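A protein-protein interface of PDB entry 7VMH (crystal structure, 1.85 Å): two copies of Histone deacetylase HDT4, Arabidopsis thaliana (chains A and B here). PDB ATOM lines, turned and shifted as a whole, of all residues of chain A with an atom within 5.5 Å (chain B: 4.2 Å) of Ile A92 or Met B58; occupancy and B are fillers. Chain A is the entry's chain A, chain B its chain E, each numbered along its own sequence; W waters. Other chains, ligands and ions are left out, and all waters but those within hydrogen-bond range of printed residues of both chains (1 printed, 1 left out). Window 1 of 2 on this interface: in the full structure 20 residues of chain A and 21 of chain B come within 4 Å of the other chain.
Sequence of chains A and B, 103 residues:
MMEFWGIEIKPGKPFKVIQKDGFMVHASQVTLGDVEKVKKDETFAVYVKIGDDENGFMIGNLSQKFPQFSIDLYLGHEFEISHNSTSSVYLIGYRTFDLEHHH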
ATOM      1  N   PHE A   4      18.935   4.094 -22.408  1.00  0.00           N
ATOM      2  CA  PHE A   4      20.017   3.480 -23.155  1.00  0.00           C
ATOM      3  C   PHE A   4      21.160   3.144 -22.229  1.00  0.00           C
ATOM      4  O   PHE A   4      21.505   3.906 -21.328  1.00  0.00           O
ATOM      5  CB  PHE A   4      20.534   4.408 -24.256  1.00  0.00           C
ATOM      6  CG  PHE A   4      21.725   3.855 -24.987  1.00  0.00           C
ATOM      7  CD1 PHE A   4      21.551   3.059 -26.107  1.00  0.00           C
ATOM      8  CD2 PHE A   4      22.989   4.083 -24.532  1.00  0.00           C
ATOM      9  CE1 PHE A   4      22.618   2.530 -26.789  1.00  0.00           C
ATOM     10  CE2 PHE A   4      24.096   3.550 -25.178  1.00  0.00           C
ATOM     11  CZ  PHE A   4      23.914   2.787 -26.323  1.00  0.00           C
ATOM     12  N   TRP A   5      21.760   1.985 -22.473  1.00  0.00           N
ATOM     13  CA  TRP A   5      22.883   1.486 -21.693  1.00  0.00           C
ATOM     14  C   TRP A   5      23.850   0.866 -22.687  1.00  0.00           C
ATOM     15  O   TRP A   5      23.420   0.115 -23.573  1.00  0.00           O
ATOM     16  CB  TRP A   5      22.411   0.459 -20.700  1.00  0.00           C
ATOM     17  CG  TRP A   5      23.532  -0.165 -19.886  1.00  0.00           C
ATOM     18  CD1 TRP A   5      24.033   0.306 -18.718  1.00  0.00           C
ATOM     19  CD2 TRP A   5      24.255  -1.339 -20.188  1.00  0.00           C
ATOM     20  NE1 TRP A   5      25.041  -0.510 -18.291  1.00  0.00           N
ATOM     21  CE2 TRP A   5      25.216  -1.506 -19.186  1.00  0.00           C
ATOM     22  CE3 TRP A   5      24.212  -2.254 -21.230  1.00  0.00           C
ATOM     23  CZ2 TRP A   5      26.072  -2.620 -19.142  1.00  0.00           C
ATOM     24  CZ3 TRP A   5      25.137  -3.356 -21.194  1.00  0.00           C
ATOM     25  CH2 TRP A   5      26.044  -3.473 -20.165  1.00  0.00           C
ATOM     26  N   GLY A   6      25.136   1.131 -22.524  1.00  0.00           N
ATOM     27  CA  GLY A   6      26.156   0.558 -23.387  1.00  0.00           C
ATOM     28  C   GLY A   6      27.535   0.499 -22.762  1.00  0.00           C
ATOM     29  O   GLY A   6      27.893   1.356 -21.944  1.00  0.00           O
ATOM     30  N   ILE A   7      28.297  -0.544 -23.102  1.00  0.00           N
ATOM     31  CA  ILE A   7      29.700  -0.665 -22.668  1.00  0.00           C
ATOM     32  C   ILE A   7      30.549  -1.104 -23.855  1.00  0.00           C
ATOM     33  O   ILE A   7      30.080  -1.815 -24.758  1.00  0.00           O
ATOM     34  CB  ILE A   7      29.877  -1.635 -21.502  1.00  0.00           C
ATOM     35  CG1 ILE A   7      29.344  -3.035 -21.829  1.00  0.00           C
ATOM     36  CG2 ILE A   7      29.151  -1.107 -20.264  1.00  0.00           C
ATOM     37  CD1 ILE A   7      29.749  -4.084 -20.758  1.00  0.00           C
ATOM     38  N   HIS A  26      19.135  -4.793 -19.576  1.00  0.00           N
ATOM     39  CA  HIS A  26      18.694  -5.639 -20.683  1.00  0.00           C
ATOM     40  C   HIS A  26      19.734  -5.467 -21.783  1.00  0.00           C
ATOM     41  O   HIS A  26      19.825  -4.399 -22.445  1.00  0.00           O
ATOM     42  CB  HIS A  26      17.336  -5.201 -21.254  1.00  0.00           C
ATOM     43  CG  HIS A  26      16.897  -6.052 -22.413  1.00  0.00           C
ATOM     44  ND1 HIS A  26      17.272  -5.811 -23.732  1.00  0.00           N
ATOM     45  CD2 HIS A  26      16.198  -7.207 -22.411  1.00  0.00           C
ATOM     46  CE1 HIS A  26      16.791  -6.785 -24.491  1.00  0.00           C
ATOM     47  NE2 HIS A  26      16.118  -7.629 -23.719  1.00  0.00           N
ATOM     48  N   ALA A  27      20.510  -6.504 -22.048  1.00  0.00           N
ATOM     49  CA  ALA A  27      21.421  -6.513 -23.156  1.00  0.00           C
ATOM     50  C   ALA A  27      20.636  -6.894 -24.416  1.00  0.00           C
ATOM     51  O   ALA A  27      19.869  -7.867 -24.396  1.00  0.00           O
ATOM     52  CB  ALA A  27      22.529  -7.514 -22.904  1.00  0.00           C
ATOM     53  N   SER A  28      20.790  -6.095 -25.478  1.00  0.00           N
ATOM     54  CA  SER A  28      20.085  -6.244 -26.724  1.00  0.00           C
ATOM     55  C   SER A  28      20.939  -6.600 -27.918  1.00  0.00           C
ATOM     56  O   SER A  28      20.461  -7.233 -28.853  1.00  0.00           O
ATOM     57  CB  SER A  28      19.350  -4.941 -27.066  1.00  0.00           C
ATOM     58  OG  SER A  28      18.382  -4.661 -26.077  1.00  0.00           O
ATOM     59  N   GLN A  29      22.177  -6.114 -27.955  1.00  0.00           N
ATOM     60  CA  GLN A  29      22.995  -6.182 -29.157  1.00  0.00           C
ATOM     61  C   GLN A  29      24.471  -6.293 -28.784  1.00  0.00           C
ATOM     62  O   GLN A  29      24.931  -5.632 -27.861  1.00  0.00           O
ATOM     63  CB  GLN A  29      22.743  -4.950 -30.035  1.00  0.00           C
ATOM     64  CG  GLN A  29      23.463  -4.962 -31.377  1.00  0.00           C
ATOM     65  CD  GLN A  29      22.717  -5.719 -32.464  1.00  0.00           C
ATOM     66  OE1 GLN A  29      21.834  -6.527 -32.181  1.00  0.00           O
ATOM     67  NE2 GLN A  29      23.034  -5.415 -33.724  1.00  0.00           N
ATOM     68  N   VAL A  30      25.207  -7.136 -29.513  1.00  0.00           N
ATOM     69  CA  VAL A  30      26.632  -7.388 -29.343  1.00  0.00           C
ATOM     70  C   VAL A  30      27.269  -7.231 -30.697  1.00  0.00           C
ATOM     71  O   VAL A  30      26.901  -7.911 -31.613  1.00  0.00           O
ATOM     72  CB  VAL A  30      26.894  -8.814 -28.826  1.00  0.00           C
ATOM     73  CG1 VAL A  30      28.379  -9.052 -28.594  1.00  0.00           C
ATOM     74  CG2 VAL A  30      26.039  -9.118 -27.589  1.00  0.00           C
ATOM     75  N   THR A  31      28.214  -6.304 -30.831  1.00  0.00           N
ATOM     76  CA  THR A  31      28.792  -5.904 -32.101  1.00  0.00           C
ATOM     77  C   THR A  31      30.323  -5.932 -32.057  1.00  0.00           C
ATOM     78  O   THR A  31      30.948  -5.468 -31.082  1.00  0.00           O
ATOM     79  CB  THR A  31      28.325  -4.484 -32.461  1.00  0.00           C
ATOM     80  OG1 THR A  31      26.887  -4.467 -32.537  1.00  0.00           O
ATOM     81  CG2 THR A  31      28.908  -4.048 -33.778  1.00  0.00           C
ATOM     82  N   LEU A  32      30.916  -6.498 -33.119  1.00  0.00           N
ATOM     83  CA  LEU A  32      32.353  -6.557 -33.292  1.00  0.00           C
ATOM     84  C   LEU A  32      32.881  -5.229 -33.806  1.00  0.00           C
ATOM     85  O   LEU A  32      32.400  -4.738 -34.835  1.00  0.00           O
ATOM     86  CB  LEU A  32      32.687  -7.654 -34.299  1.00  0.00           C
ATOM     87  CG  LEU A  32      34.182  -7.984 -34.480  1.00  0.00           C
ATOM     88  CD1 LEU A  32      34.897  -8.421 -33.227  1.00  0.00           C
ATOM     89  CD2 LEU A  32      34.257  -9.065 -35.544  1.00  0.00           C
ATOM     90  N   GLY A  33      33.853  -4.646 -33.098  1.00  0.00           N
ATOM     91  CA  GLY A  33      34.541  -3.454 -33.557  1.00  0.00           C
ATOM     92  C   GLY A  33      35.599  -3.721 -34.606  1.00  0.00           C
ATOM     93  O   GLY A  33      36.108  -4.839 -34.722  1.00  0.00           O
ATOM     94  N   ASP A  34      35.940  -2.675 -35.377  1.00  0.00           N
ATOM     95  CA  ASP A  34      37.059  -2.707 -36.318  1.00  0.00           C
ATOM     96  C   ASP A  34      37.051  -3.931 -37.174  1.00  0.00           C
ATOM     97  O   ASP A  34      38.073  -4.635 -37.254  1.00  0.00           O
ATOM     98  CB  ASP A  34      38.399  -2.654 -35.590  1.00  0.00           C
ATOM     99  CG  ASP A  34      38.639  -1.327 -34.897  1.00  0.00           C
ATOM    100  OD1 ASP A  34      38.217  -0.307 -35.424  1.00  0.00           O
ATOM    101  OD2 ASP A  34      39.234  -1.256 -33.791  1.00  0.00           O
ATOM    102  N   TYR A  90      31.224  -4.190 -28.464  1.00  0.00           N
ATOM    103  CA  TYR A  90      30.215  -3.254 -27.896  1.00  0.00           C
ATOM    104  C   TYR A  90      28.979  -4.048 -27.510  1.00  0.00           C
ATOM    105  O   TYR A  90      28.393  -4.674 -28.394  1.00  0.00           O
ATOM    106  CB  TYR A  90      29.834  -2.174 -28.899  1.00  0.00           C
ATOM    107  CG  TYR A  90      30.965  -1.273 -29.304  1.00  0.00           C
ATOM    108  CD1 TYR A  90      31.804  -1.609 -30.356  1.00  0.00           C
ATOM    109  CD2 TYR A  90      31.225  -0.109 -28.604  1.00  0.00           C
ATOM    110  CE1 TYR A  90      32.856  -0.784 -30.736  1.00  0.00           C
ATOM    111  CE2 TYR A  90      32.269   0.733 -28.959  1.00  0.00           C
ATOM    112  CZ  TYR A  90      33.076   0.392 -30.036  1.00  0.00           C
ATOM    113  OH  TYR A  90      34.081   1.211 -30.438  1.00  0.00           O
ATOM    114  N   LEU A  91      28.613  -3.976 -26.225  1.00  0.00           N
ATOM    115  CA  LEU A  91      27.388  -4.559 -25.760  1.00  0.00           C
ATOM    116  C   LEU A  91      26.488  -3.395 -25.405  1.00  0.00           C
ATOM    117  O   LEU A  91      26.863  -2.556 -24.559  1.00  0.00           O
ATOM    118  CB  LEU A  91      27.679  -5.421 -24.541  1.00  0.00           C
ATOM    119  CG  LEU A  91      26.515  -6.135 -23.904  1.00  0.00           C
ATOM    120  CD1 LEU A  91      26.044  -7.217 -24.811  1.00  0.00           C
ATOM    121  CD2 LEU A  91      26.864  -6.754 -22.556  1.00  0.00           C
ATOM    122  N   ILE A  92      25.297  -3.346 -26.007  1.00  0.00           N
ATOM    123  CA  ILE A  92      24.344  -2.266 -25.758  1.00  0.00           C
ATOM    124  C   ILE A  92      22.954  -2.817 -25.477  1.00  0.00           C
ATOM    125  O   ILE A  92      22.614  -3.959 -25.783  1.00  0.00           O
ATOM    126  CB  ILE A  92      24.308  -1.219 -26.910  1.00  0.00           C
ATOM    127  CG1 ILE A  92      23.728  -1.843 -28.150  1.00  0.00           C
ATOM    128  CG2 ILE A  92      25.689  -0.676 -27.197  1.00  0.00           C
ATOM    129  CD1 ILE A  92      23.589  -0.958 -29.347  1.00  0.00           C
ATOM    130  N   GLY A  93      22.117  -1.960 -24.886  1.00  0.00           N
ATOM    131  CA  GLY A  93      20.764  -2.315 -24.521  1.00  0.00           C
ATOM    132  C   GLY A  93      20.139  -1.171 -23.784  1.00  0.00           C
ATOM    133  O   GLY A  93      20.331  -0.037 -24.148  1.00  0.00           O
ATOM    134  N   TYR A  94      19.441  -1.480 -22.704  1.00  0.00           N
ATOM    135  CA  TYR A  94      18.780  -0.472 -21.849  1.00  0.00           C
ATOM    136  C   TYR A  94      18.749  -0.954 -20.412  1.00  0.00           C
ATOM    137  O   TYR A  94      18.768  -2.146 -20.129  1.00  0.00           O
ATOM    138  CB  TYR A  94      17.398  -0.135 -22.386  1.00  0.00           C
ATOM    139  CG  TYR A  94      16.529  -1.291 -22.786  1.00  0.00           C
ATOM    140  CD1 TYR A  94      15.605  -1.859 -21.925  1.00  0.00           C
ATOM    141  CD2 TYR A  94      16.576  -1.756 -24.089  1.00  0.00           C
ATOM    142  CE1 TYR A  94      14.773  -2.898 -22.334  1.00  0.00           C
ATOM    143  CE2 TYR A  94      15.755  -2.792 -24.517  1.00  0.00           C
ATOM    144  CZ  TYR A  94      14.852  -3.365 -23.627  1.00  0.00           C
ATOM    145  OH  TYR A  94      14.082  -4.394 -24.115  1.00  0.00           O
ATOM    146  N   ALA B  45      30.629   0.376 -40.142  1.00  0.00           N
ATOM    147  CA  ALA B  45      30.232   0.519 -38.779  1.00  0.00           C
ATOM    148  C   ALA B  45      29.126   1.561 -38.603  1.00  0.00           C
ATOM    149  O   ALA B  45      29.163   2.588 -39.245  1.00  0.00           O
ATOM    150  CB  ALA B  45      31.481   0.925 -38.004  1.00  0.00           C
ATOM    151  N   VAL B  46      28.167   1.259 -37.741  1.00  0.00           N
ATOM    152  CA  VAL B  46      27.088   2.179 -37.329  1.00  0.00           C
ATOM    153  C   VAL B  46      27.245   2.426 -35.845  1.00  0.00           C
ATOM    154  O   VAL B  46      27.289   1.486 -35.048  1.00  0.00           O
ATOM    155  CB  VAL B  46      25.697   1.625 -37.628  1.00  0.00           C
ATOM    156  CG1 VAL B  46      24.655   2.689 -37.402  1.00  0.00           C
ATOM    157  CG2 VAL B  46      25.613   1.087 -39.089  1.00  0.00           C
ATOM    158  N   TYR B  47      27.340   3.705 -35.471  1.00  0.00           N
ATOM    159  CA  TYR B  47      27.544   4.196 -34.095  1.00  0.00           C
ATOM    160  C   TYR B  47      26.357   5.034 -33.599  1.00  0.00           C
ATOM    161  O   TYR B  47      25.686   5.717 -34.391  1.00  0.00           O
ATOM    162  CB  TYR B  47      28.807   5.054 -34.038  1.00  0.00           C
ATOM    163  CG  TYR B  47      30.077   4.267 -33.856  1.00  0.00           C
ATOM    164  CD1 TYR B  47      30.842   3.813 -34.917  1.00  0.00           C
ATOM    165  CD2 TYR B  47      30.523   4.014 -32.577  1.00  0.00           C
ATOM    166  CE1 TYR B  47      32.025   3.104 -34.703  1.00  0.00           C
ATOM    167  CE2 TYR B  47      31.695   3.309 -32.338  1.00  0.00           C
ATOM    168  CZ  TYR B  47      32.468   2.880 -33.401  1.00  0.00           C
ATOM    169  OH  TYR B  47      33.595   2.150 -33.112  1.00  0.00           O
ATOM    170  N   PHE B  57      28.964   4.153 -29.198  1.00  0.00           N
ATOM    171  CA  PHE B  57      28.834   2.704 -29.063  1.00  0.00           C
ATOM    172  C   PHE B  57      28.376   2.203 -30.376  1.00  0.00           C
ATOM    173  O   PHE B  57      27.537   2.814 -31.032  1.00  0.00           O
ATOM    174  CB  PHE B  57      27.793   2.335 -28.004  1.00  0.00           C
ATOM    175  CG  PHE B  57      28.124   2.864 -26.668  1.00  0.00           C
ATOM    176  CD1 PHE B  57      28.929   2.127 -25.801  1.00  0.00           C
ATOM    177  CD2 PHE B  57      27.662   4.112 -26.261  1.00  0.00           C
ATOM    178  CE1 PHE B  57      29.269   2.624 -24.557  1.00  0.00           C
ATOM    179  CE2 PHE B  57      27.991   4.604 -25.009  1.00  0.00           C
ATOM    180  CZ  PHE B  57      28.811   3.870 -24.167  1.00  0.00           C
ATOM    181  N   MET B  58      28.977   1.097 -30.836  1.00  0.00           N
ATOM    182  CA  MET B  58      28.508   0.486 -32.081  1.00  0.00           C
ATOM    183  C   MET B  58      27.163  -0.155 -31.856  1.00  0.00           C
ATOM    184  O   MET B  58      26.950  -0.875 -30.871  1.00  0.00           O
ATOM    185  CB  MET B  58      29.474  -0.561 -32.602  1.00  0.00           C
ATOM    186  CG  MET B  58      30.640   0.071 -33.269  1.00  0.00           C
ATOM    187  SD  MET B  58      31.687  -1.193 -34.016  1.00  0.00           S
ATOM    188  CE  MET B  58      30.856  -1.449 -35.540  1.00  0.00           C
ATOM    189  N   ILE B  59      26.250   0.083 -32.801  1.00  0.00           N
ATOM    190  CA  ILE B  59      24.965  -0.636 -32.816  1.00  0.00           C
ATOM    191  C   ILE B  59      24.947  -1.826 -33.779  1.00  0.00           C
ATOM    192  O   ILE B  59      24.069  -2.701 -33.669  1.00  0.00           O
ATOM    193  CB  ILE B  59      23.760   0.272 -33.000  1.00  0.00           C
ATOM    194  CG1 ILE B  59      23.681   0.766 -34.432  1.00  0.00           C
ATOM    195  CG2 ILE B  59      23.826   1.414 -31.978  1.00  0.00           C
ATOM    196  CD1 ILE B  59      22.437   1.602 -34.706  1.00  0.00           C
ATOM    197  N   GLY B  60      25.928  -1.885 -34.674  1.00  0.00           N
ATOM    198  CA  GLY B  60      26.078  -2.971 -35.612  1.00  0.00           C
ATOM    199  C   GLY B  60      26.933  -2.596 -36.793  1.00  0.00           C
ATOM    200  O   GLY B  60      27.475  -1.482 -36.899  1.00  0.00           O
ATOM    201  N   ASN B  61      27.166  -3.577 -37.655  1.00  0.00           N
ATOM    202  CA  ASN B  61      27.862  -3.440 -38.912  1.00  0.00           C
ATOM    203  C   ASN B  61      26.953  -3.775 -40.011  1.00  0.00           C
ATOM    204  O   ASN B  61      25.989  -4.514 -39.798  1.00  0.00           O
ATOM    205  CB  ASN B  61      29.076  -4.425 -38.974  1.00  0.00           C
ATOM    206  CG  ASN B  61      30.110  -4.093 -37.946  1.00  0.00           C
ATOM    207  OD1 ASN B  61      30.934  -3.215 -38.182  1.00  0.00           O
ATOM    208  ND2 ASN B  61      30.137  -4.826 -36.882  1.00  0.00           N
ATOM    209  N   LEU B  73      16.316  -1.396 -29.305  1.00  0.00           N
ATOM    210  CA  LEU B  73      16.951  -0.300 -28.570  1.00  0.00           C
ATOM    211  C   LEU B  73      15.988   0.812 -28.288  1.00  0.00           C
ATOM    212  O   LEU B  73      15.265   1.208 -29.187  1.00  0.00           O
ATOM    213  CB  LEU B  73      18.048   0.283 -29.455  1.00  0.00           C
ATOM    214  CG  LEU B  73      19.503   0.495 -29.049  1.00  0.00           C
ATOM    215  CD1 LEU B  73      20.079  -0.676 -28.232  1.00  0.00           C
ATOM    216  CD2 LEU B  73      20.300   0.819 -30.331  1.00  0.00           C
HETATM  217  O   HOH W   1      33.565  -2.522 -37.448  1.00  0.00           O
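Printed residues of chain B that touch a printed residue of chain A: Tyr B47, Phe B57, Met B58, Ile B59, Gly B60, Asn B61 and Leu B73. Hydrophobic or aromatic side chains of chain B within 4 Å of the printed part of chain A: Tyr B47, Phe B57, Met B58, Ile B59 and Leu B73. Printed residues of chain A that touch a printed residue of chain B: Phe A4, Gly A6, Ile A7, Gln A29, Thr A31, Leu A32, Gly A33, Tyr A90 and Ile A92. Among the printed residues, 18 pairs touch across the chains. Among the printed residues, no Asp or Glu carboxylate lies within 4 Å of a Lys or Arg side-chain nitrogen of the other chain.
Ile A92 touches four residues of chain B. Met B58 touches five residues of chain A. Of the printed residues of chain A, Tyr B47 touches Tyr A90. Printed residues of chain B within 4 Å of Tyr A90: Tyr B47, Phe B57 and Met B58. Of the printed residues of chain B, Gly A6 touches Phe B57. His A26 touches none of the printed residues of chain B. The nearest printed residue of chain B that does not touch Ile A92 is Gly B60 (5.9 Å). The nearest printed residue of chain B that does not touch Gln A29 is Gly B60 (4.3 Å).
Phe A4 touches Phe B57. Gly A6 touches Phe B57 (O to CE1, 3.2 Å). CE1 of Phe B57 touches N of Ile A7, at 3.6 Å. Thr A31 touches Ile B59. CG2 of Thr A31 touches ND2 of Asn B61, at 3.4 Å. Met B58 touches Gly A33. Tyr A90 touches Phe B57. Phe B57 touches Ile A92. Ile A92 touches Met B58. Ile A92 touches Ile B59 (CD1 to CG2, 3.6 Å).
The backbone carbonyl oxygen (O) of Ile B59 is in hydrogen-bond range of the side-chain amide nitrogen (NE2) of Gln A29, at 2.9 Å. OG1 of Thr A31 lies within hydrogen-bond range of N of Gly B60, 3.5 Å away. ND2 of Asn B61 lies within hydrogen-bond range of O of Leu A32, at 3.1 Å. The side-chain hydroxyl (OH) of Tyr A90 sits at hydrogen-bond distance from the side-chain hydroxyl (OH) of Tyr B47, 2.9 Å away. O of Leu A32 sits close to SD of Met B58.
No position is printed for both chains. Of the 18 pairs that touch across the chains among the printed residues, none has its exchanged pair printed and touching as well.
N of Ile A7 is in hydrogen-bond range of O of Leu A91, 2.9 Å away. The backbone NH (N) of Ser A28 sits at hydrogen-bond distance from the backbone carbonyl oxygen (O) of Ile A92, 2.8 Å away. O of Gln A29 sits at hydrogen-bond distance from N of Ile A92 (3.0 Å). The backbone carbonyl oxygen (O) of Thr A31 is in hydrogen-bond range of the backbone NH (N) of Tyr A90. The backbone carbonyl oxygen (O) of Val B46 sits at hydrogen-bond distance from the backbone NH (N) of Ile B59 (2.8 Å). N of Val B46 is in hydrogen-bond range of O of Gly B60, at 2.9 Å.
Water W1 lies within hydrogen-bond range of the side-chain amide oxygen of Asn B61 (2.8 Å) and the backbone NH of Asp A34 (3.2 Å).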
